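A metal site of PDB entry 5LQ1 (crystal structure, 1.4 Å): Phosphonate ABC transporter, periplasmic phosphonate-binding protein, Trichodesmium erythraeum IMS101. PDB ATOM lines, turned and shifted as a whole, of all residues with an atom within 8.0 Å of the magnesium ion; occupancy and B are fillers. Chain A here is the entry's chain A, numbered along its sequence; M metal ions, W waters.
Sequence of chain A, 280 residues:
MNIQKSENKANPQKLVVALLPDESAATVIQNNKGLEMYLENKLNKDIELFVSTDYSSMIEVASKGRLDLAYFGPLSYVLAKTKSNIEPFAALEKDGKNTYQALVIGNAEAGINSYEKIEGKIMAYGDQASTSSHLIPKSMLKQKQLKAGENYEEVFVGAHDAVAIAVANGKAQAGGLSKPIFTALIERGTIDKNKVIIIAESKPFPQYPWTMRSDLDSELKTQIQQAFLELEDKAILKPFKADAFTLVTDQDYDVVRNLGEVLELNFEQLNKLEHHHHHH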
ATOM      1  N   LYS A  14     -24.126 -23.350 -22.006  1.00  0.00           N
ATOM      2  CA  LYS A  14     -23.580 -24.695 -22.193  1.00  0.00           C
ATOM      3  C   LYS A  14     -24.678 -25.608 -22.705  1.00  0.00           C
ATOM      4  O   LYS A  14     -25.838 -25.478 -22.333  1.00  0.00           O
ATOM      5  CB  LYS A  14     -22.914 -25.274 -20.926  1.00  0.00           C
ATOM      6  CG  LYS A  14     -23.865 -25.708 -19.844  1.00  0.00           C
ATOM      7  CD  LYS A  14     -23.138 -26.455 -18.748  1.00  0.00           C
ATOM      8  CE  LYS A  14     -24.026 -26.616 -17.521  1.00  0.00           C
ATOM      9  NZ  LYS A  14     -25.225 -27.449 -17.785  1.00  0.00           N
ATOM     10  N   LEU A  15     -24.275 -26.532 -23.569  1.00  0.00           N
ATOM     11  CA  LEU A  15     -25.191 -27.484 -24.200  1.00  0.00           C
ATOM     12  C   LEU A  15     -24.963 -28.882 -23.617  1.00  0.00           C
ATOM     13  O   LEU A  15     -23.831 -29.368 -23.635  1.00  0.00           O
ATOM     14  CB  LEU A  15     -24.977 -27.529 -25.711  1.00  0.00           C
ATOM     15  CG  LEU A  15     -25.285 -26.254 -26.514  1.00  0.00           C
ATOM     16  CD1 LEU A  15     -24.927 -26.428 -27.972  1.00  0.00           C
ATOM     17  CD2 LEU A  15     -26.747 -25.846 -26.338  1.00  0.00           C
ATOM     18  N   LYS A  33     -14.824 -36.689 -29.621  1.00  0.00           N
ATOM     19  CA  LYS A  33     -14.011 -35.559 -29.086  1.00  0.00           C
ATOM     20  C   LYS A  33     -13.753 -34.465 -30.150  1.00  0.00           C
ATOM     21  O   LYS A  33     -13.898 -33.255 -29.861  1.00  0.00           O
ATOM     22  CB  LYS A  33     -12.704 -36.044 -28.443  1.00  0.00           C
ATOM     23  CG  LYS A  33     -12.919 -36.621 -27.038  1.00  0.00           C
ATOM     24  CD  LYS A  33     -13.143 -35.531 -25.978  1.00  0.00           C
ATOM     25  CE  LYS A  33     -13.570 -36.070 -24.627  1.00  0.00           C
ATOM     26  NZ  LYS A  33     -14.663 -35.263 -23.988  1.00  0.00           N
ATOM     27  N   GLU A  36     -17.046 -32.526 -30.878  1.00  0.00           N
ATOM     28  CA  GLU A  36     -17.333 -31.671 -29.725  1.00  0.00           C
ATOM     29  C   GLU A  36     -16.541 -30.354 -29.789  1.00  0.00           C
ATOM     30  O   GLU A  36     -17.090 -29.261 -29.616  1.00  0.00           O
ATOM     31  CB  GLU A  36     -16.992 -32.405 -28.411  1.00  0.00           C
ATOM     32  CG  GLU A  36     -17.290 -31.593 -27.155  1.00  0.00           C
ATOM     33  CD  GLU A  36     -16.856 -32.270 -25.882  1.00  0.00           C
ATOM     34  OE1 GLU A  36     -16.216 -33.352 -25.931  1.00  0.00           O
ATOM     35  OE2 GLU A  36     -17.137 -31.684 -24.808  1.00  0.00           O
ATOM     36  N   MET A  37     -15.259 -30.483 -30.043  1.00  0.00           N
ATOM     37  CA  MET A  37     -14.313 -29.314 -30.058  1.00  0.00           C
ATOM     38  C   MET A  37     -14.681 -28.370 -31.206  1.00  0.00           C
ATOM     39  O   MET A  37     -14.768 -27.151 -31.008  1.00  0.00           O
ATOM     40  CB  MET A  37     -12.880 -29.807 -30.216  1.00  0.00           C
ATOM     41  CG  MET A  37     -11.784 -28.814 -29.832  1.00  0.00           C
ATOM     42  SD  MET A  37     -10.127 -29.554 -29.968  1.00  0.00           S
ATOM     43  CE  MET A  37     -10.317 -30.952 -28.833  1.00  0.00           C
ATOM     44  N   GLU A  40     -18.034 -26.580 -30.216  1.00  0.00           N
ATOM     45  CA  GLU A  40     -17.802 -25.579 -29.178  1.00  0.00           C
ATOM     46  C   GLU A  40     -17.213 -24.277 -29.745  1.00  0.00           C
ATOM     47  O   GLU A  40     -17.677 -23.188 -29.431  1.00  0.00           O
ATOM     48  CB  GLU A  40     -16.884 -26.121 -28.103  1.00  0.00           C
ATOM     49  CG  GLU A  40     -17.601 -27.130 -27.226  1.00  0.00           C
ATOM     50  CD  GLU A  40     -16.687 -27.807 -26.234  1.00  0.00           C
ATOM     51  OE1 GLU A  40     -15.547 -28.149 -26.574  1.00  0.00           O
ATOM     52  OE2 GLU A  40     -17.136 -28.022 -25.088  1.00  0.00           O
ATOM     53  N   LYS A  45     -19.962 -22.045 -27.505  1.00  0.00           N
ATOM     54  CA  LYS A  45     -20.626 -22.614 -26.312  1.00  0.00           C
ATOM     55  C   LYS A  45     -19.821 -23.767 -25.791  1.00  0.00           C
ATOM     56  O   LYS A  45     -19.055 -24.380 -26.524  1.00  0.00           O
ATOM     57  CB  LYS A  45     -22.055 -23.090 -26.586  1.00  0.00           C
ATOM     58  CG  LYS A  45     -22.937 -21.947 -26.968  1.00  0.00           C
ATOM     59  CD  LYS A  45     -24.391 -22.329 -27.017  1.00  0.00           C
ATOM     60  CE  LYS A  45     -25.217 -21.159 -27.476  1.00  0.00           C
ATOM     61  NZ  LYS A  45     -25.349 -20.049 -26.518  1.00  0.00           N
ATOM     62  N   ASP A  46     -19.983 -24.012 -24.500  1.00  0.00           N
ATOM     63  CA  ASP A  46     -19.422 -25.182 -23.874  1.00  0.00           C
ATOM     64  C   ASP A  46     -20.381 -26.362 -24.126  1.00  0.00           C
ATOM     65  O   ASP A  46     -21.588 -26.215 -24.051  1.00  0.00           O
ATOM     66  CB  ASP A  46     -19.223 -24.959 -22.378  1.00  0.00           C
ATOM     67  CG  ASP A  46     -18.243 -23.828 -22.091  1.00  0.00           C
ATOM     68  OD1 ASP A  46     -17.092 -23.897 -22.556  1.00  0.00           O
ATOM     69  OD2 ASP A  46     -18.633 -22.878 -21.397  1.00  0.00           O
ATOM     70  N   ILE A  47     -19.813 -27.509 -24.421  1.00  0.00           N
ATOM     71  CA  ILE A  47     -20.602 -28.748 -24.569  1.00  0.00           C
ATOM     72  C   ILE A  47     -20.253 -29.691 -23.424  1.00  0.00           C
ATOM     73  O   ILE A  47     -19.106 -29.869 -23.079  1.00  0.00           O
ATOM     74  CB  ILE A  47     -20.344 -29.401 -25.933  1.00  0.00           C
ATOM     75  CG1 ILE A  47     -21.157 -28.658 -27.005  1.00  0.00           C
ATOM     76  CG2 ILE A  47     -20.731 -30.882 -25.918  1.00  0.00           C
ATOM     77  CD1 ILE A  47     -20.887 -29.116 -28.419  1.00  0.00           C
ATOM     78  N   GLU A  48     -21.286 -30.325 -22.860  1.00  0.00           N
ATOM     79  CA  GLU A  48     -21.104 -31.321 -21.823  1.00  0.00           C
ATOM     80  C   GLU A  48     -21.823 -32.600 -22.257  1.00  0.00           C
ATOM     81  O   GLU A  48     -23.041 -32.614 -22.512  1.00  0.00           O
ATOM     82  CB  GLU A  48     -21.585 -30.755 -20.501  1.00  0.00           C
ATOM     83  CG  GLU A  48     -20.713 -29.525 -20.141  1.00  0.00           C
ATOM     84  CD  GLU A  48     -20.866 -29.007 -18.733  1.00  0.00           C
ATOM     85  OE1 GLU A  48     -21.729 -29.493 -17.979  1.00  0.00           O
ATOM     86  OE2 GLU A  48     -20.114 -28.080 -18.381  1.00  0.00           O
ATOM     87  N   LEU A  49     -21.025 -33.648 -22.381  1.00  0.00           N
ATOM     88  CA  LEU A  49     -21.454 -34.925 -22.946  1.00  0.00           C
ATOM     89  C   LEU A  49     -22.095 -35.822 -21.893  1.00  0.00           C
ATOM     90  O   LEU A  49     -21.687 -35.818 -20.727  1.00  0.00           O
ATOM     91  CB  LEU A  49     -20.288 -35.663 -23.627  1.00  0.00           C
ATOM     92  CG  LEU A  49     -19.572 -34.999 -24.789  1.00  0.00           C
ATOM     93  CD1 LEU A  49     -18.443 -35.872 -25.320  1.00  0.00           C
ATOM     94  CD2 LEU A  49     -20.556 -34.670 -25.913  1.00  0.00           C
HETATM   95 MG    MG M   1     -17.184 -29.619 -23.634  1.00  0.00          MG
HETATM   96  O   HOH W   1     -17.014 -28.047 -22.212  1.00  0.00           O
HETATM   97  O   HOH W   2     -14.927 -29.263 -23.921  1.00  0.00           O
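The backbone carbonyl oxygen of Glu 40 sits at hydrogen-bond distance from the backbone NH of Lys 45 (3.2 Å). OE1 of Glu 36 is in salt-bridge range of NZ of Lys 33 (3.1 Å).
The magnesium ion is bound by the backbone carbonyl oxygen of Ile 47, water W1, the side-chain carboxylate of Glu 40, water W2 and the side-chain carboxylate of Glu 36.
Along chain A the residues within 4 Å of the magnesium ion span positions 36 to 47.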
